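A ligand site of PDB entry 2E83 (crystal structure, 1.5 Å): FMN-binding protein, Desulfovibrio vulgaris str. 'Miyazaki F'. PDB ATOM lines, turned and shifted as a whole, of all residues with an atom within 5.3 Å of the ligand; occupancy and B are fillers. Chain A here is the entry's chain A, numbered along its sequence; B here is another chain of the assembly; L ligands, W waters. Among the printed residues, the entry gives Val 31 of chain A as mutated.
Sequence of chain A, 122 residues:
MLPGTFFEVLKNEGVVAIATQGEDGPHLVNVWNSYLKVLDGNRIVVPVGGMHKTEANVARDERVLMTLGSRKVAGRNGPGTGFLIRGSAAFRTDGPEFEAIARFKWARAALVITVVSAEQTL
Water W6 lies within hydrogen-bond range of the side-chain hydroxyl (OG1) of Thr 121 of chain B (2.7 Å), an oxygen (O3) of the ligand (2.7 Å) and the side-chain amide oxygen (OD1) of Asn 30 (2.7 Å). Water W2 bridges an oxygen (O4) of the ligand and the backbone carbonyl oxygen of Thr 121 of chain B. Water W3 bridges a nitrogen (N1) of the ligand (3.4 Å) and the backbone NH (N) of Gly 50 (3.4 Å).
O9 of the ligand lies within hydrogen-bond range of N of Thr 54, at 2.8 Å. An oxygen (O9) of the ligand sits at hydrogen-bond distance from the side-chain hydroxyl (OG1) of Thr 54, 2.7 Å away. N of Gly 49 lies within hydrogen-bond range of O1 of the ligand (2.7 Å). An oxygen (O7) of the ligand sits at hydrogen-bond distance from a ring nitrogen (NE2) of His 27 (2.8 Å). N of Asn 30 is in hydrogen-bond range of O3 of the ligand (2.8 Å). The backbone carbonyl oxygen of Asn 30 lies close to an oxygen (O3) of the ligand, at 3.5 Å. The backbone NH (N) of Met 51 is in hydrogen-bond range of an oxygen (O5) of the ligand, at 2.8 Å. N of Lys 53 is in hydrogen-bond range of O8 of the ligand (2.9 Å). The backbone NH (N) of Gly 50 is in hydrogen-bond range of an oxygen (O1) of the ligand (2.9 Å). O8 of the ligand sits at hydrogen-bond distance from N of His 52 (2.9 Å). The backbone carbonyl oxygen of Pro 47 is in hydrogen-bond range of a nitrogen (N2) of the ligand (3.1 Å).
Merely in contact with the ligand: Val 29 (3.5 Å), Val 31 (3.3 Å), Trp 32 (3.4 Å), Tyr 35 (3.1 Å), Val 48 (3.7 Å), Trp 106 (3.4 Å), Gly 82 of chain B (3.4 Å), Thr 121 of chain B (3.3 Å) and Leu 122 of chain B (3.7 Å). Hydrophobic or aromatic side chains within 4 Å of the ligand: His 27, Val 29, Val 31, Trp 32, Tyr 35, Met 51, His 52, Trp 106 and Leu 122 of chain B. Of the 24 residues printed, 18 come within 4 Å of the ligand.
N of Thr 121 of chain B is in hydrogen-bond range of O of Gly 82 of chain B (3.0 Å). OG1 of Thr 81 of chain B lies within hydrogen-bond range of O of Leu 122 of chain B (2.7 Å).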
ATOM      1  N   VAL A  15      21.261  -1.715  17.196  1.00  0.00           N
ATOM      2  CA  VAL A  15      21.283  -0.865  16.023  1.00  0.00           C
ATOM      3  C   VAL A  15      21.571   0.570  16.437  1.00  0.00           C
ATOM      4  O   VAL A  15      20.820   1.174  17.195  1.00  0.00           O
ATOM      5  CB  VAL A  15      19.935  -0.925  15.285  1.00  0.00           C
ATOM      6  CG1 VAL A  15      19.948   0.003  14.078  1.00  0.00           C
ATOM      7  CG2 VAL A  15      19.638  -2.349  14.845  1.00  0.00           C
ATOM      8  N   HIS A  27      18.365  13.103   7.441  1.00  0.00           N
ATOM      9  CA  HIS A  27      18.634  11.759   6.958  1.00  0.00           C
ATOM     10  C   HIS A  27      19.057  10.895   8.131  1.00  0.00           C
ATOM     11  O   HIS A  27      19.509  11.415   9.163  1.00  0.00           O
ATOM     12  CB  HIS A  27      19.735  11.758   5.896  1.00  0.00           C
ATOM     13  CG  HIS A  27      19.838  10.469   5.142  1.00  0.00           C
ATOM     14  ND1 HIS A  27      18.745   9.819   4.622  1.00  0.00           N
ATOM     15  CD2 HIS A  27      20.908   9.696   4.835  1.00  0.00           C
ATOM     16  CE1 HIS A  27      19.131   8.712   4.023  1.00  0.00           C
ATOM     17  NE2 HIS A  27      20.446   8.616   4.131  1.00  0.00           N
ATOM     18  N   VAL A  29      20.800   6.928   9.091  1.00  0.00           N
ATOM     19  CA  VAL A  29      21.403   5.646   8.715  1.00  0.00           C
ATOM     20  C   VAL A  29      21.854   4.880   9.950  1.00  0.00           C
ATOM     21  O   VAL A  29      21.783   5.379  11.071  1.00  0.00           O
ATOM     22  CB  VAL A  29      22.620   5.835   7.780  1.00  0.00           C
ATOM     23  CG1 VAL A  29      22.188   6.554   6.505  1.00  0.00           C
ATOM     24  CG2 VAL A  29      23.721   6.623   8.493  1.00  0.00           C
ATOM     25  N   ASN A  30      22.326   3.656   9.729  1.00  0.00           N
ATOM     26  CA  ASN A  30      22.619   2.747  10.827  1.00  0.00           C
ATOM     27  C   ASN A  30      23.997   2.131  10.763  1.00  0.00           C
ATOM     28  O   ASN A  30      24.604   2.037   9.695  1.00  0.00           O
ATOM     29  CB  ASN A  30      21.576   1.634  10.869  1.00  0.00           C
ATOM     30  CG  ASN A  30      20.173   2.163  11.031  1.00  0.00           C
ATOM     31  OD1 ASN A  30      19.335   2.030  10.143  1.00  0.00           O
ATOM     32  ND2 ASN A  30      19.925   2.791  12.171  1.00  0.00           N
ATOM     33  N   VAL A  31      24.489   1.706  11.928  1.00  0.00           N
ATOM     34  CA  VAL A  31      25.599   0.764  12.041  1.00  0.00           C
ATOM     35  C   VAL A  31      25.283  -0.131  13.238  1.00  0.00           C
ATOM     36  O   VAL A  31      24.404   0.192  14.038  1.00  0.00           O
ATOM     37  CB  VAL A  31      26.940   1.483  12.283  1.00  0.00           C
ATOM     38  CG1 VAL A  31      27.248   2.423  11.131  1.00  0.00           C
ATOM     39  CG2 VAL A  31      26.883   2.257  13.588  1.00  0.00           C
ATOM     40  N   TRP A  32      25.987  -1.254  13.359  1.00  0.00           N
ATOM     41  CA  TRP A  32      25.784  -2.140  14.496  1.00  0.00           C
ATOM     42  C   TRP A  32      26.570  -1.655  15.709  1.00  0.00           C
ATOM     43  O   TRP A  32      27.672  -1.116  15.564  1.00  0.00           O
ATOM     44  CB  TRP A  32      26.239  -3.564  14.155  1.00  0.00           C
ATOM     45  CG  TRP A  32      25.464  -4.211  13.068  1.00  0.00           C
ATOM     46  CD1 TRP A  32      25.911  -4.483  11.804  1.00  0.00           C
ATOM     47  CD2 TRP A  32      24.141  -4.747  13.143  1.00  0.00           C
ATOM     48  NE1 TRP A  32      24.946  -5.152  11.088  1.00  0.00           N
ATOM     49  CE2 TRP A  32      23.842  -5.332  11.897  1.00  0.00           C
ATOM     50  CE3 TRP A  32      23.169  -4.783  14.157  1.00  0.00           C
ATOM     51  CZ2 TRP A  32      22.613  -5.954  11.627  1.00  0.00           C
ATOM     52  CZ3 TRP A  32      21.946  -5.401  13.894  1.00  0.00           C
ATOM     53  CH2 TRP A  32      21.686  -5.981  12.633  1.00  0.00           C
ATOM     54  N   TYR A  35      30.217  -2.547  15.896  1.00  0.00           N
ATOM     55  CA  TYR A  35      31.117  -1.950  14.911  1.00  0.00           C
ATOM     56  C   TYR A  35      31.823  -0.700  15.430  1.00  0.00           C
ATOM     57  O   TYR A  35      32.860  -0.304  14.897  1.00  0.00           O
ATOM     58  CB  TYR A  35      30.353  -1.576  13.646  1.00  0.00           C
ATOM     59  CG  TYR A  35      30.002  -2.724  12.729  1.00  0.00           C
ATOM     60  CD1 TYR A  35      29.467  -2.470  11.459  1.00  0.00           C
ATOM     61  CD2 TYR A  35      30.188  -4.048  13.105  1.00  0.00           C
ATOM     62  CE1 TYR A  35      29.155  -3.499  10.586  1.00  0.00           C
ATOM     63  CE2 TYR A  35      29.870  -5.102  12.235  1.00  0.00           C
ATOM     64  CZ  TYR A  35      29.351  -4.816  10.978  1.00  0.00           C
ATOM     65  OH  TYR A  35      29.028  -5.826  10.102  1.00  0.00           O
ATOM     66  N   PRO A  47      32.814   2.034  10.583  1.00  0.00           N
ATOM     67  CA  PRO A  47      33.165   1.638   9.212  1.00  0.00           C
ATOM     68  C   PRO A  47      32.107   2.092   8.227  1.00  0.00           C
ATOM     69  O   PRO A  47      30.907   1.878   8.449  1.00  0.00           O
ATOM     70  CB  PRO A  47      33.259   0.113   9.299  1.00  0.00           C
ATOM     71  CG  PRO A  47      32.336  -0.244  10.419  1.00  0.00           C
ATOM     72  CD  PRO A  47      32.448   0.878  11.420  1.00  0.00           C
ATOM     73  N   VAL A  48      32.548   2.712   7.143  1.00  0.00           N
ATOM     74  CA  VAL A  48      31.630   3.204   6.117  1.00  0.00           C
ATOM     75  C   VAL A  48      31.719   2.347   4.858  1.00  0.00           C
ATOM     76  O   VAL A  48      32.753   2.290   4.199  1.00  0.00           O
ATOM     77  CB  VAL A  48      31.970   4.663   5.732  1.00  0.00           C
ATOM     78  CG1 VAL A  48      31.063   5.119   4.590  1.00  0.00           C
ATOM     79  CG2 VAL A  48      31.791   5.566   6.946  1.00  0.00           C
ATOM     80  N   GLY A  49      30.607   1.670   4.543  1.00  0.00           N
ATOM     81  CA  GLY A  49      30.488   0.992   3.272  1.00  0.00           C
ATOM     82  C   GLY A  49      29.710   1.854   2.292  1.00  0.00           C
ATOM     83  O   GLY A  49      30.187   2.138   1.190  1.00  0.00           O
ATOM     84  N   GLY A  50      28.515   2.258   2.696  1.00  0.00           N
ATOM     85  CA  GLY A  50      27.717   3.164   1.885  1.00  0.00           C
ATOM     86  C   GLY A  50      27.828   4.587   2.376  1.00  0.00           C
ATOM     87  O   GLY A  50      28.836   5.254   2.159  1.00  0.00           O
ATOM     88  N   MET A  51      26.779   5.058   3.039  1.00  0.00           N
ATOM     89  CA  MET A  51      26.738   6.398   3.628  1.00  0.00           C
ATOM     90  C   MET A  51      27.116   7.493   2.649  1.00  0.00           C
ATOM     91  O   MET A  51      27.828   8.439   2.998  1.00  0.00           O
ATOM     92  CB  MET A  51      27.638   6.457   4.859  1.00  0.00           C
ATOM     93  CG  MET A  51      27.200   5.531   5.968  1.00  0.00           C
ATOM     94  SD  MET A  51      27.858   6.033   7.573  1.00  0.00           S
ATOM     95  CE  MET A  51      27.365   4.647   8.578  1.00  0.00           C
ATOM     96  N   HIS A  52      26.631   7.381   1.419  1.00  0.00           N
ATOM     97  CA  HIS A  52      26.920   8.388   0.411  1.00  0.00           C
ATOM     98  C   HIS A  52      26.082   9.640   0.588  1.00  0.00           C
ATOM     99  O   HIS A  52      26.575  10.757   0.461  1.00  0.00           O
ATOM    100  CB  HIS A  52      26.701   7.796  -0.984  1.00  0.00           C
ATOM    101  CG  HIS A  52      27.661   6.700  -1.315  1.00  0.00           C
ATOM    102  ND1 HIS A  52      28.995   6.929  -1.575  1.00  0.00           N
ATOM    103  CD2 HIS A  52      27.488   5.355  -1.397  1.00  0.00           C
ATOM    104  CE1 HIS A  52      29.609   5.781  -1.794  1.00  0.00           C
ATOM    105  NE2 HIS A  52      28.719   4.810  -1.701  1.00  0.00           N
ATOM    106  N   LYS A  53      24.799   9.460   0.907  1.00  0.00           N
ATOM    107  CA  LYS A  53      23.948  10.621   1.189  1.00  0.00           C
ATOM    108  C   LYS A  53      24.402  11.252   2.495  1.00  0.00           C
ATOM    109  O   LYS A  53      24.462  12.481   2.617  1.00  0.00           O
ATOM    110  CB  LYS A  53      22.481  10.201   1.308  1.00  0.00           C
ATOM    111  CG  LYS A  53      21.543  11.382   1.467  1.00  0.00           C
ATOM    112  CD  LYS A  53      20.094  10.959   1.628  1.00  0.00           C
ATOM    113  CE  LYS A  53      19.167  12.178   1.621  1.00  0.00           C
ATOM    114  NZ  LYS A  53      19.624  13.240   2.567  1.00  0.00           N
ATOM    115  N   THR A  54      24.742  10.402   3.458  1.00  0.00           N
ATOM    116  CA  THR A  54      25.216  10.869   4.746  1.00  0.00           C
ATOM    117  C   THR A  54      26.506  11.685   4.612  1.00  0.00           C
ATOM    118  O   THR A  54      26.637  12.730   5.243  1.00  0.00           O
ATOM    119  CB  THR A  54      25.441   9.660   5.692  1.00  0.00           C
ATOM    120  OG1 THR A  54      24.181   9.039   5.964  1.00  0.00           O
ATOM    121  CG2 THR A  54      26.066  10.098   7.004  1.00  0.00           C
ATOM    122  N   GLU A  55      27.435  11.221   3.789  1.00  0.00           N
ATOM    123  CA  GLU A  55      28.691  11.942   3.609  1.00  0.00           C
ATOM    124  C   GLU A  55      28.469  13.304   2.968  1.00  0.00           C
ATOM    125  O   GLU A  55      29.096  14.296   3.358  1.00  0.00           O
ATOM    126  CB  GLU A  55      29.681  11.140   2.766  1.00  0.00           C
ATOM    127  CG  GLU A  55      31.019  11.844   2.608  1.00  0.00           C
ATOM    128  CD  GLU A  55      32.066  11.022   1.866  1.00  0.00           C
ATOM    129  OE1 GLU A  55      31.733   9.922   1.363  1.00  0.00           O
ATOM    130  OE2 GLU A  55      33.224  11.481   1.804  1.00  0.00           O
ATOM    131  N   TRP A 106      35.126  -4.191   3.625  1.00  0.00           N
ATOM    132  CA  TRP A 106      34.105  -3.529   2.831  1.00  0.00           C
ATOM    133  C   TRP A 106      34.065  -2.021   3.078  1.00  0.00           C
ATOM    134  O   TRP A 106      33.367  -1.292   2.372  1.00  0.00           O
ATOM    135  CB  TRP A 106      32.720  -4.131   3.120  1.00  0.00           C
ATOM    136  CG  TRP A 106      32.408  -4.287   4.581  1.00  0.00           C
ATOM    137  CD1 TRP A 106      32.546  -5.426   5.328  1.00  0.00           C
ATOM    138  CD2 TRP A 106      31.886  -3.289   5.459  1.00  0.00           C
ATOM    139  NE1 TRP A 106      32.126  -5.191   6.619  1.00  0.00           N
ATOM    140  CE2 TRP A 106      31.718  -3.891   6.724  1.00  0.00           C
ATOM    141  CE3 TRP A 106      31.529  -1.941   5.304  1.00  0.00           C
ATOM    142  CZ2 TRP A 106      31.212  -3.187   7.831  1.00  0.00           C
ATOM    143  CZ3 TRP A 106      31.025  -1.247   6.402  1.00  0.00           C
ATOM    144  CH2 TRP A 106      30.871  -1.876   7.646  1.00  0.00           C
ATOM    145  N   LEU B  68      15.128   0.862  12.496  1.00  0.00           N
ATOM    146  CA  LEU B  68      15.100  -0.206  13.488  1.00  0.00           C
ATOM    147  C   LEU B  68      15.674  -1.453  12.832  1.00  0.00           C
ATOM    148  O   LEU B  68      15.765  -1.530  11.600  1.00  0.00           O
ATOM    149  CB  LEU B  68      13.662  -0.484  13.952  1.00  0.00           C
ATOM    150  CG  LEU B  68      12.688  -1.127  12.960  1.00  0.00           C
ATOM    151  CD1 LEU B  68      11.437  -1.582  13.705  1.00  0.00           C
ATOM    152  CD2 LEU B  68      12.328  -0.125  11.869  1.00  0.00           C
ATOM    153  N   GLY B  69      16.070  -2.419  13.640  1.00  0.00           N
ATOM    154  CA  GLY B  69      16.635  -3.637  13.076  1.00  0.00           C
ATOM    155  C   GLY B  69      16.873  -4.698  14.131  1.00  0.00           C
ATOM    156  O   GLY B  69      16.503  -4.531  15.298  1.00  0.00           O
ATOM    157  N   THR B  81      19.476  -7.486   9.922  1.00  0.00           N
ATOM    158  CA  THR B  81      18.878  -6.586   8.965  1.00  0.00           C
ATOM    159  C   THR B  81      18.216  -5.410   9.661  1.00  0.00           C
ATOM    160  O   THR B  81      18.156  -5.357  10.887  1.00  0.00           O
ATOM    161  CB  THR B  81      17.837  -7.320   8.073  1.00  0.00           C
ATOM    162  OG1 THR B  81      17.446  -6.471   6.989  1.00  0.00           O
ATOM    163  CG2 THR B  81      16.604  -7.691   8.892  1.00  0.00           C
ATOM    164  N   GLY B  82      17.712  -4.467   8.868  1.00  0.00           N
ATOM    165  CA  GLY B  82      16.979  -3.357   9.423  1.00  0.00           C
ATOM    166  C   GLY B  82      16.308  -2.533   8.345  1.00  0.00           C
ATOM    167  O   GLY B  82      16.446  -2.836   7.160  1.00  0.00           O
ATOM    168  N   PHE B  83      15.595  -1.492   8.756  1.00  0.00           N
ATOM    169  CA  PHE B  83      14.744  -0.739   7.852  1.00  0.00           C
ATOM    170  C   PHE B  83      14.879   0.761   8.032  1.00  0.00           C
ATOM    171  O   PHE B  83      15.071   1.243   9.154  1.00  0.00           O
ATOM    172  CB  PHE B  83      13.276  -1.119   8.066  1.00  0.00           C
ATOM    173  CG  PHE B  83      12.914  -2.470   7.527  1.00  0.00           C
ATOM    174  CD1 PHE B  83      13.135  -3.607   8.286  1.00  0.00           C
ATOM    175  CD2 PHE B  83      12.368  -2.598   6.253  1.00  0.00           C
ATOM    176  CE1 PHE B  83      12.827  -4.870   7.785  1.00  0.00           C
ATOM    177  CE2 PHE B  83      12.063  -3.854   5.746  1.00  0.00           C
ATOM    178  CZ  PHE B  83      12.289  -4.987   6.513  1.00  0.00           C
ATOM    179  N   THR B 121      17.411  -1.949   4.441  1.00  0.00           N
ATOM    180  CA  THR B 121      18.672  -1.349   4.063  1.00  0.00           C
ATOM    181  C   THR B 121      19.880  -2.260   4.279  1.00  0.00           C
ATOM    182  O   THR B 121      21.021  -1.828   4.176  1.00  0.00           O
ATOM    183  CB  THR B 121      18.905  -0.037   4.830  1.00  0.00           C
ATOM    184  OG1 THR B 121      18.633  -0.254   6.219  1.00  0.00           O
ATOM    185  CG2 THR B 121      17.992   1.059   4.300  1.00  0.00           C
ATOM    186  N   LEU B 122      19.604  -3.527   4.592  1.00  0.00           N
ATOM    187  CA  LEU B 122      20.669  -4.507   4.763  1.00  0.00           C
ATOM    188  C   LEU B 122      20.136  -5.898   4.440  1.00  0.00           C
ATOM    189  O   LEU B 122      18.948  -6.143   4.721  1.00  0.00           O
ATOM    190  CB  LEU B 122      21.182  -4.462   6.203  1.00  0.00           C
ATOM    191  CG  LEU B 122      22.352  -5.355   6.611  1.00  0.00           C
ATOM    192  CD1 LEU B 122      23.592  -5.010   5.801  1.00  0.00           C
ATOM    193  CD2 LEU B 122      22.621  -5.158   8.098  1.00  0.00           C
ATOM    194  OXT LEU B 122      20.914  -6.732   3.909  1.00  0.00           O
HETATM  195  N1  LIG L   1      26.179   1.136   6.289  1.00  0.00           N
HETATM  196  C1  LIG L   1      27.536   1.377   6.405  1.00  0.00           C
HETATM  197  O1  LIG L   1      28.141   2.082   5.599  1.00  0.00           O
HETATM  198  N2  LIG L   1      28.217   0.805   7.490  1.00  0.00           N
HETATM  199  C2  LIG L   1      27.639   0.011   8.465  1.00  0.00           C
HETATM  200  O2  LIG L   1      28.325  -0.456   9.405  1.00  0.00           O
HETATM  201  C3  LIG L   1      26.212  -0.235   8.343  1.00  0.00           C
HETATM  202  N3  LIG L   1      25.584  -0.997   9.269  1.00  0.00           N
HETATM  203  C4  LIG L   1      24.202  -1.165   9.183  1.00  0.00           C
HETATM  204  C5  LIG L   1      23.508  -1.885  10.192  1.00  0.00           C
HETATM  205  C6  LIG L   1      22.109  -2.082  10.144  1.00  0.00           C
HETATM  206  C7  LIG L   1      21.425  -2.845  11.245  1.00  0.00           C
HETATM  207  C8  LIG L   1      21.392  -1.530   9.028  1.00  0.00           C
HETATM  208  C9  LIG L   1      19.864  -1.714   8.937  1.00  0.00           C
HETATM  209  C10 LIG L   1      22.046  -0.818   8.047  1.00  0.00           C
HETATM  210  C11 LIG L   1      23.445  -0.598   8.071  1.00  0.00           C
HETATM  211  N4  LIG L   1      24.167   0.148   7.095  1.00  0.00           N
HETATM  212  C12 LIG L   1      25.546   0.370   7.207  1.00  0.00           C
HETATM  213  C13 LIG L   1      23.461   0.770   5.949  1.00  0.00           C
HETATM  214  C14 LIG L   1      23.158   2.252   6.230  1.00  0.00           C
HETATM  215  O3  LIG L   1      22.164   2.368   7.232  1.00  0.00           O
HETATM  216  C15 LIG L   1      22.748   3.023   4.980  1.00  0.00           C
HETATM  217  O4  LIG L   1      21.514   2.432   4.492  1.00  0.00           O
HETATM  218  C16 LIG L   1      23.764   2.967   3.845  1.00  0.00           C
HETATM  219  O5  LIG L   1      25.133   3.125   4.291  1.00  0.00           O
HETATM  220  C17 LIG L   1      23.496   4.050   2.810  1.00  0.00           C
HETATM  221  O6  LIG L   1      23.778   5.338   3.404  1.00  0.00           O
HETATM  222  P1  LIG L   1      23.197   6.679   2.751  1.00  0.00           P
HETATM  223  O7  LIG L   1      21.692   6.563   2.752  1.00  0.00           O
HETATM  224  O8  LIG L   1      23.745   6.779   1.327  1.00  0.00           O
HETATM  225  O9  LIG L   1      23.727   7.764   3.641  1.00  0.00           O
HETATM  226  O   HOH W   1      19.790   6.754   0.861  1.00  0.00           O
HETATM  227  O   HOH W   2      21.384   0.903   2.212  1.00  0.00           O
HETATM  228  O   HOH W   3      27.559  -0.808   3.916  1.00  0.00           O
HETATM  229  O   HOH W   4      23.044   5.250  -0.742  1.00  0.00           O
HETATM  230  O   HOH W   5      25.383   0.062   2.770  1.00  0.00           O
HETATM  231  O   HOH W   6      19.529   1.929   7.466  1.00  0.00           O
HETATM  232  O   HOH W   7      20.060   4.587   3.735  1.00  0.00           O
